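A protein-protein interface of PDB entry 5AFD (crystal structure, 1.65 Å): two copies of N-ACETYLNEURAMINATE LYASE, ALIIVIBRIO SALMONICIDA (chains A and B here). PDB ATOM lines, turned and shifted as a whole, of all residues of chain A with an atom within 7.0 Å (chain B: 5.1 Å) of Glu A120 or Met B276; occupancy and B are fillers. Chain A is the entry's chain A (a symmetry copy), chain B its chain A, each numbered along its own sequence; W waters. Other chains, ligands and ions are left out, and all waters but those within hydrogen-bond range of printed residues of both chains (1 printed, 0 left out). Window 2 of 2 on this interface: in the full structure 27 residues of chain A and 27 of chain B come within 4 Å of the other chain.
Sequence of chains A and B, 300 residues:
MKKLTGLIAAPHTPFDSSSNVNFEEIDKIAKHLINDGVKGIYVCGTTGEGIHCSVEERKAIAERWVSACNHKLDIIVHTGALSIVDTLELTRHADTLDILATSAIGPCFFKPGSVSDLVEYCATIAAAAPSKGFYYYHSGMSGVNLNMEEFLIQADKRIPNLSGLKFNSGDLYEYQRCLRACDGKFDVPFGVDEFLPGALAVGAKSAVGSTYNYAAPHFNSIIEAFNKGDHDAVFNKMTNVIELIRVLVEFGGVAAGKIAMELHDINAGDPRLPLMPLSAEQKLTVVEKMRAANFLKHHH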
ATOM      1  N   GLY A 113      18.453  21.303 -12.207  1.00  0.00           N
ATOM      2  CA  GLY A 113      19.566  21.260 -11.218  1.00  0.00           C
ATOM      3  C   GLY A 113      19.962  19.835 -10.825  1.00  0.00           C
ATOM      4  O   GLY A 113      20.989  19.615 -10.178  1.00  0.00           O
ATOM      5  N   SER A 114      19.167  18.847 -11.257  1.00  0.00           N
ATOM      6  CA  SER A 114      19.509  17.444 -11.021  1.00  0.00           C
ATOM      7  C   SER A 114      19.034  16.586 -12.240  1.00  0.00           C
ATOM      8  O   SER A 114      18.090  16.979 -12.983  1.00  0.00           O
ATOM      9  CB  SER A 114      18.878  16.905  -9.747  1.00  0.00           C
ATOM     10  OG  SER A 114      17.442  16.780  -9.934  1.00  0.00           O
ATOM     11  N   VAL A 115      19.580  15.361 -12.326  1.00  0.00           N
ATOM     12  CA  VAL A 115      19.161  14.409 -13.358  1.00  0.00           C
ATOM     13  C   VAL A 115      17.643  14.163 -13.205  1.00  0.00           C
ATOM     14  O   VAL A 115      16.874  14.181 -14.219  1.00  0.00           O
ATOM     15  CB  VAL A 115      19.946  13.109 -13.232  1.00  0.00           C
ATOM     16  CG1 VAL A 115      19.441  12.007 -14.167  1.00  0.00           C
ATOM     17  CG2 VAL A 115      21.414  13.441 -13.605  1.00  0.00           C
ATOM     18  N   SER A 116      17.201  13.938 -11.955  1.00  0.00           N
ATOM     19  CA  SER A 116      15.778  13.675 -11.732  1.00  0.00           C
ATOM     20  C   SER A 116      14.890  14.766 -12.244  1.00  0.00           C
ATOM     21  O   SER A 116      13.871  14.474 -12.831  1.00  0.00           O
ATOM     22  CB  SER A 116      15.454  13.396 -10.246  1.00  0.00           C
ATOM     23  OG  SER A 116      14.130  12.996 -10.103  1.00  0.00           O
ATOM     24  N   ASP A 117      15.306  16.022 -12.062  1.00  0.00           N
ATOM     25  CA  ASP A 117      14.494  17.150 -12.484  1.00  0.00           C
ATOM     26  C   ASP A 117      14.478  17.160 -14.002  1.00  0.00           C
ATOM     27  O   ASP A 117      13.467  17.440 -14.635  1.00  0.00           O
ATOM     28  CB  ASP A 117      15.079  18.464 -11.949  1.00  0.00           C
ATOM     29  CG  ASP A 117      14.890  18.639 -10.463  1.00  0.00           C
ATOM     30  OD1 ASP A 117      14.199  17.827  -9.809  1.00  0.00           O
ATOM     31  OD2 ASP A 117      15.422  19.616  -9.981  1.00  0.00           O
ATOM     32  N   LEU A 118      15.636  16.917 -14.628  1.00  0.00           N
ATOM     33  CA  LEU A 118      15.672  16.927 -16.099  1.00  0.00           C
ATOM     34  C   LEU A 118      14.790  15.785 -16.708  1.00  0.00           C
ATOM     35  O   LEU A 118      14.075  15.967 -17.744  1.00  0.00           O
ATOM     36  CB  LEU A 118      17.124  16.783 -16.586  1.00  0.00           C
ATOM     37  CG  LEU A 118      17.288  16.630 -18.109  1.00  0.00           C
ATOM     38  CD1 LEU A 118      16.847  17.923 -18.812  1.00  0.00           C
ATOM     39  CD2 LEU A 118      18.757  16.528 -18.512  1.00  0.00           C
ATOM     40  N   VAL A 119      14.792  14.644 -16.031  1.00  0.00           N
ATOM     41  CA  VAL A 119      13.975  13.484 -16.464  1.00  0.00           C
ATOM     42  C   VAL A 119      12.497  13.904 -16.371  1.00  0.00           C
ATOM     43  O   VAL A 119      11.737  13.666 -17.312  1.00  0.00           O
ATOM     44  CB  VAL A 119      14.252  12.242 -15.634  1.00  0.00           C
ATOM     45  CG1 VAL A 119      13.156  11.214 -15.958  1.00  0.00           C
ATOM     46  CG2 VAL A 119      15.656  11.664 -15.943  1.00  0.00           C
ATOM     47  N   GLU A 120      12.094  14.560 -15.295  1.00  0.00           N
ATOM     48  CA  GLU A 120      10.673  14.992 -15.204  1.00  0.00           C
ATOM     49  C   GLU A 120      10.282  15.959 -16.326  1.00  0.00           C
ATOM     50  O   GLU A 120       9.201  15.843 -16.953  1.00  0.00           O
ATOM     51  CB  GLU A 120      10.331  15.605 -13.842  1.00  0.00           C
ATOM     52  CG  GLU A 120       8.936  16.205 -13.827  1.00  0.00           C
ATOM     53  CD  GLU A 120       7.851  15.222 -13.482  1.00  0.00           C
ATOM     54  OE1 GLU A 120       8.131  14.147 -12.907  1.00  0.00           O
ATOM     55  OE2 GLU A 120       6.675  15.603 -13.709  1.00  0.00           O
ATOM     56  N   TYR A 121      11.149  16.922 -16.621  1.00  0.00           N
ATOM     57  CA  TYR A 121      10.887  17.867 -17.736  1.00  0.00           C
ATOM     58  C   TYR A 121      10.784  17.095 -19.095  1.00  0.00           C
ATOM     59  O   TYR A 121       9.795  17.248 -19.849  1.00  0.00           O
ATOM     60  CB  TYR A 121      12.119  18.814 -17.778  1.00  0.00           C
ATOM     61  CG  TYR A 121      12.132  19.790 -18.962  1.00  0.00           C
ATOM     62  CD1 TYR A 121      11.191  20.856 -18.978  1.00  0.00           C
ATOM     63  CD2 TYR A 121      12.986  19.645 -20.056  1.00  0.00           C
ATOM     64  CE1 TYR A 121      11.154  21.802 -20.033  1.00  0.00           C
ATOM     65  CE2 TYR A 121      12.937  20.585 -21.138  1.00  0.00           C
ATOM     66  CZ  TYR A 121      12.024  21.667 -21.100  1.00  0.00           C
ATOM     67  OH  TYR A 121      11.954  22.601 -22.150  1.00  0.00           O
ATOM     68  N   CYS A 122      11.779  16.205 -19.348  1.00  0.00           N
ATOM     69  CA  CYS A 122      11.728  15.457 -20.642  1.00  0.00           C
ATOM     70  C   CYS A 122      10.488  14.503 -20.727  1.00  0.00           C
ATOM     71  O   CYS A 122       9.950  14.326 -21.803  1.00  0.00           O
ATOM     72  CB  CYS A 122      12.978  14.622 -20.763  1.00  0.00           C
ATOM     73  SG  CYS A 122      14.407  15.638 -21.219  1.00  0.00           S
ATOM     74  N   ALA A 123      10.093  13.957 -19.581  1.00  0.00           N
ATOM     75  CA  ALA A 123       8.970  12.964 -19.537  1.00  0.00           C
ATOM     76  C   ALA A 123       7.722  13.769 -19.888  1.00  0.00           C
ATOM     77  O   ALA A 123       6.849  13.256 -20.614  1.00  0.00           O
ATOM     78  CB  ALA A 123       8.919  12.304 -18.157  1.00  0.00           C
ATOM     79  N   THR A 124       7.596  15.012 -19.443  1.00  0.00           N
ATOM     80  CA  THR A 124       6.352  15.760 -19.724  1.00  0.00           C
ATOM     81  C   THR A 124       6.253  16.065 -21.228  1.00  0.00           C
ATOM     82  O   THR A 124       5.174  16.032 -21.860  1.00  0.00           O
ATOM     83  CB  THR A 124       6.423  17.067 -18.875  1.00  0.00           C
ATOM     84  OG1 THR A 124       6.449  16.706 -17.460  1.00  0.00           O
ATOM     85  CG2 THR A 124       5.218  17.955 -19.148  1.00  0.00           C
ATOM     86  N   ILE A 125       7.359  16.503 -21.821  1.00  0.00           N
ATOM     87  CA  ILE A 125       7.486  16.713 -23.244  1.00  0.00           C
ATOM     88  C   ILE A 125       7.210  15.443 -24.076  1.00  0.00           C
ATOM     89  O   ILE A 125       6.363  15.498 -24.958  1.00  0.00           O
ATOM     90  CB  ILE A 125       8.835  17.363 -23.632  1.00  0.00           C
ATOM     91  CG1 ILE A 125       8.924  18.733 -22.853  1.00  0.00           C
ATOM     92  CG2 ILE A 125       8.953  17.525 -25.191  1.00  0.00           C
ATOM     93  CD1 ILE A 125      10.387  19.237 -22.963  1.00  0.00           C
ATOM     94  N   PHE A 151      21.179  10.335 -16.649  1.00  0.00           N
ATOM     95  CA  PHE A 151      19.941  10.678 -17.372  1.00  0.00           C
ATOM     96  C   PHE A 151      19.334   9.512 -18.166  1.00  0.00           C
ATOM     97  O   PHE A 151      18.105   9.234 -18.020  1.00  0.00           O
ATOM     98  CB  PHE A 151      20.169  11.888 -18.336  1.00  0.00           C
ATOM     99  CG  PHE A 151      18.982  12.153 -19.200  1.00  0.00           C
ATOM    100  CD1 PHE A 151      17.886  12.830 -18.640  1.00  0.00           C
ATOM    101  CD2 PHE A 151      18.921  11.664 -20.512  1.00  0.00           C
ATOM    102  CE1 PHE A 151      16.727  13.047 -19.456  1.00  0.00           C
ATOM    103  CE2 PHE A 151      17.743  11.856 -21.280  1.00  0.00           C
ATOM    104  CZ  PHE A 151      16.693  12.578 -20.768  1.00  0.00           C
ATOM    105  N   ILE A 159      10.289   7.288 -19.196  1.00  0.00           N
ATOM    106  CA  ILE A 159       9.881   7.770 -20.517  1.00  0.00           C
ATOM    107  C   ILE A 159       9.697   6.577 -21.515  1.00  0.00           C
ATOM    108  O   ILE A 159      10.693   6.054 -22.042  1.00  0.00           O
ATOM    109  CB  ILE A 159      10.927   8.814 -21.063  1.00  0.00           C
ATOM    110  CG1 ILE A 159      11.096   9.914 -20.013  1.00  0.00           C
ATOM    111  CG2 ILE A 159      10.361   9.354 -22.405  1.00  0.00           C
ATOM    112  CD1 ILE A 159      11.977  11.111 -20.480  1.00  0.00           C
ATOM    113  N   ALA B 255      10.131  29.020  -6.264  1.00  0.00           N
ATOM    114  CA  ALA B 255       9.150  28.158  -5.568  1.00  0.00           C
ATOM    115  C   ALA B 255       8.842  28.622  -4.124  1.00  0.00           C
ATOM    116  O   ALA B 255       7.661  28.734  -3.697  1.00  0.00           O
ATOM    117  CB  ALA B 255       9.571  26.708  -5.592  1.00  0.00           C
ATOM    118  N   PRO B 271       5.581  26.782  -9.371  1.00  0.00           N
ATOM    119  CA  PRO B 271       6.205  27.299 -10.609  1.00  0.00           C
ATOM    120  C   PRO B 271       5.811  26.361 -11.779  1.00  0.00           C
ATOM    121  O   PRO B 271       5.186  25.308 -11.579  1.00  0.00           O
ATOM    122  CB  PRO B 271       7.719  27.117 -10.375  1.00  0.00           C
ATOM    123  CG  PRO B 271       7.898  26.497  -9.014  1.00  0.00           C
ATOM    124  CD  PRO B 271       6.519  26.111  -8.458  1.00  0.00           C
ATOM    125  N   LEU B 273       7.273  23.901 -14.841  1.00  0.00           N
ATOM    126  CA  LEU B 273       8.450  23.206 -15.457  1.00  0.00           C
ATOM    127  C   LEU B 273       9.187  24.128 -16.416  1.00  0.00           C
ATOM    128  O   LEU B 273       8.580  24.913 -17.135  1.00  0.00           O
ATOM    129  CB  LEU B 273       7.973  21.907 -16.182  1.00  0.00           C
ATOM    130  CG  LEU B 273       7.544  20.794 -15.211  1.00  0.00           C
ATOM    131  CD1 LEU B 273       6.996  19.610 -15.999  1.00  0.00           C
ATOM    132  CD2 LEU B 273       8.790  20.331 -14.424  1.00  0.00           C
ATOM    133  N   PRO B 274      10.527  24.137 -16.377  1.00  0.00           N
ATOM    134  CA  PRO B 274      11.449  23.184 -15.698  1.00  0.00           C
ATOM    135  C   PRO B 274      11.705  23.398 -14.206  1.00  0.00           C
ATOM    136  O   PRO B 274      12.414  22.555 -13.557  1.00  0.00           O
ATOM    137  CB  PRO B 274      12.765  23.340 -16.500  1.00  0.00           C
ATOM    138  CG  PRO B 274      12.690  24.833 -16.842  1.00  0.00           C
ATOM    139  CD  PRO B 274      11.256  25.024 -17.329  1.00  0.00           C
ATOM    140  N   LEU B 275      11.112  24.466 -13.614  1.00  0.00           N
ATOM    141  CA  LEU B 275      11.176  24.580 -12.153  1.00  0.00           C
ATOM    142  C   LEU B 275      10.228  23.527 -11.523  1.00  0.00           C
ATOM    143  O   LEU B 275       9.127  23.251 -11.973  1.00  0.00           O
ATOM    144  CB  LEU B 275      10.825  25.978 -11.661  1.00  0.00           C
ATOM    145  CG  LEU B 275      11.712  27.084 -12.194  1.00  0.00           C
ATOM    146  CD1 LEU B 275      11.089  28.407 -11.829  1.00  0.00           C
ATOM    147  CD2 LEU B 275      13.062  26.922 -11.438  1.00  0.00           C
ATOM    148  N   MET B 276      10.669  22.913 -10.438  1.00  0.00           N
ATOM    149  CA  MET B 276       9.904  21.825  -9.842  1.00  0.00           C
ATOM    150  C   MET B 276       9.015  22.386  -8.699  1.00  0.00           C
ATOM    151  O   MET B 276       9.337  23.410  -8.080  1.00  0.00           O
ATOM    152  CB  MET B 276      10.892  20.799  -9.250  1.00  0.00           C
ATOM    153  CG  MET B 276      11.846  20.244 -10.272  1.00  0.00           C
ATOM    154  SD  MET B 276      10.984  19.301 -11.583  1.00  0.00           S
ATOM    155  CE  MET B 276      10.251  17.931 -10.739  1.00  0.00           C
ATOM    156  N   PRO B 277       7.910  21.698  -8.393  1.00  0.00           N
ATOM    157  CA  PRO B 277       7.049  22.074  -7.284  1.00  0.00           C
ATOM    158  C   PRO B 277       7.562  21.564  -5.957  1.00  0.00           C
ATOM    159  O   PRO B 277       8.343  20.572  -5.902  1.00  0.00           O
ATOM    160  CB  PRO B 277       5.693  21.432  -7.655  1.00  0.00           C
ATOM    161  CG  PRO B 277       6.041  20.289  -8.570  1.00  0.00           C
ATOM    162  CD  PRO B 277       7.434  20.502  -9.107  1.00  0.00           C
ATOM    163  N   LEU B 278       7.203  22.274  -4.874  1.00  0.00           N
ATOM    164  CA  LEU B 278       7.517  21.784  -3.547  1.00  0.00           C
ATOM    165  C   LEU B 278       6.407  20.788  -3.118  1.00  0.00           C
ATOM    166  O   LEU B 278       5.226  20.938  -3.565  1.00  0.00           O
ATOM    167  CB  LEU B 278       7.579  22.944  -2.542  1.00  0.00           C
ATOM    168  CG  LEU B 278       8.739  23.945  -2.840  1.00  0.00           C
ATOM    169  CD1 LEU B 278       8.510  25.193  -2.046  1.00  0.00           C
ATOM    170  CD2 LEU B 278      10.066  23.379  -2.393  1.00  0.00           C
HETATM  171  O   HOH W   1      13.395  20.304 -14.787  1.00  0.00           O
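No position is printed for both chains.
Of the 4 pairs that touch across the chains among the printed residues, none has its exchanged pair printed and touching as well.
The backbone carbonyl oxygen (O) of Glu A120 lies within hydrogen-bond range of the side-chain hydroxyl (OG1) of Thr A124 (2.9 Å).
The side-chain hydroxyl of Ser A114 is in hydrogen-bond range of the backbone NH of Asp A117.
Printed residues of chain B that touch a printed residue of chain A: Leu B273, Pro B274 and Met B276.
Hydrophobic or aromatic side chains of chain B within 4 Å of the printed part of chain A: Leu B273, Pro B274 and Met B276.
Printed residues of chain A that touch a printed residue of chain B: Asp A117, Glu A120, Tyr A121 and Thr A124.
Among the printed residues, 4 pairs touch across the chains.
Among the printed residues, no Asp or Glu carboxylate lies within 4 Å of a Lys or Arg side-chain nitrogen of the other chain.
Among the printed residues, merely in contact across the chains: Asp A117 with Met B276, Glu A120 with Met B276, Tyr A121 with Pro B274 and Thr A124 with Leu B273.
Water W1 bridges the backbone carbonyl oxygen of Pro B274 (2.7 Å) and the backbone carbonyl oxygen of Asp A117 (2.9 Å).
Printed residues of chain B within 4 Å of Glu A120: Met B276 (3.8 Å).
Printed residues of chain B within 4 Å of Tyr A121: Pro B274.
Printed residues of chain B within 4 Å of Thr A124: Leu B273 (3.3 Å).
Ala B255 touches none of the printed residues of chain A.
Of the printed residues of chain A, Leu B273 touches Thr A124.
Of the printed residues of chain A, Met B276 touches Asp A117 and Glu A120.
The nearest printed residue of chain A that does not touch Met B276 is Ser A116 (5.4 Å).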
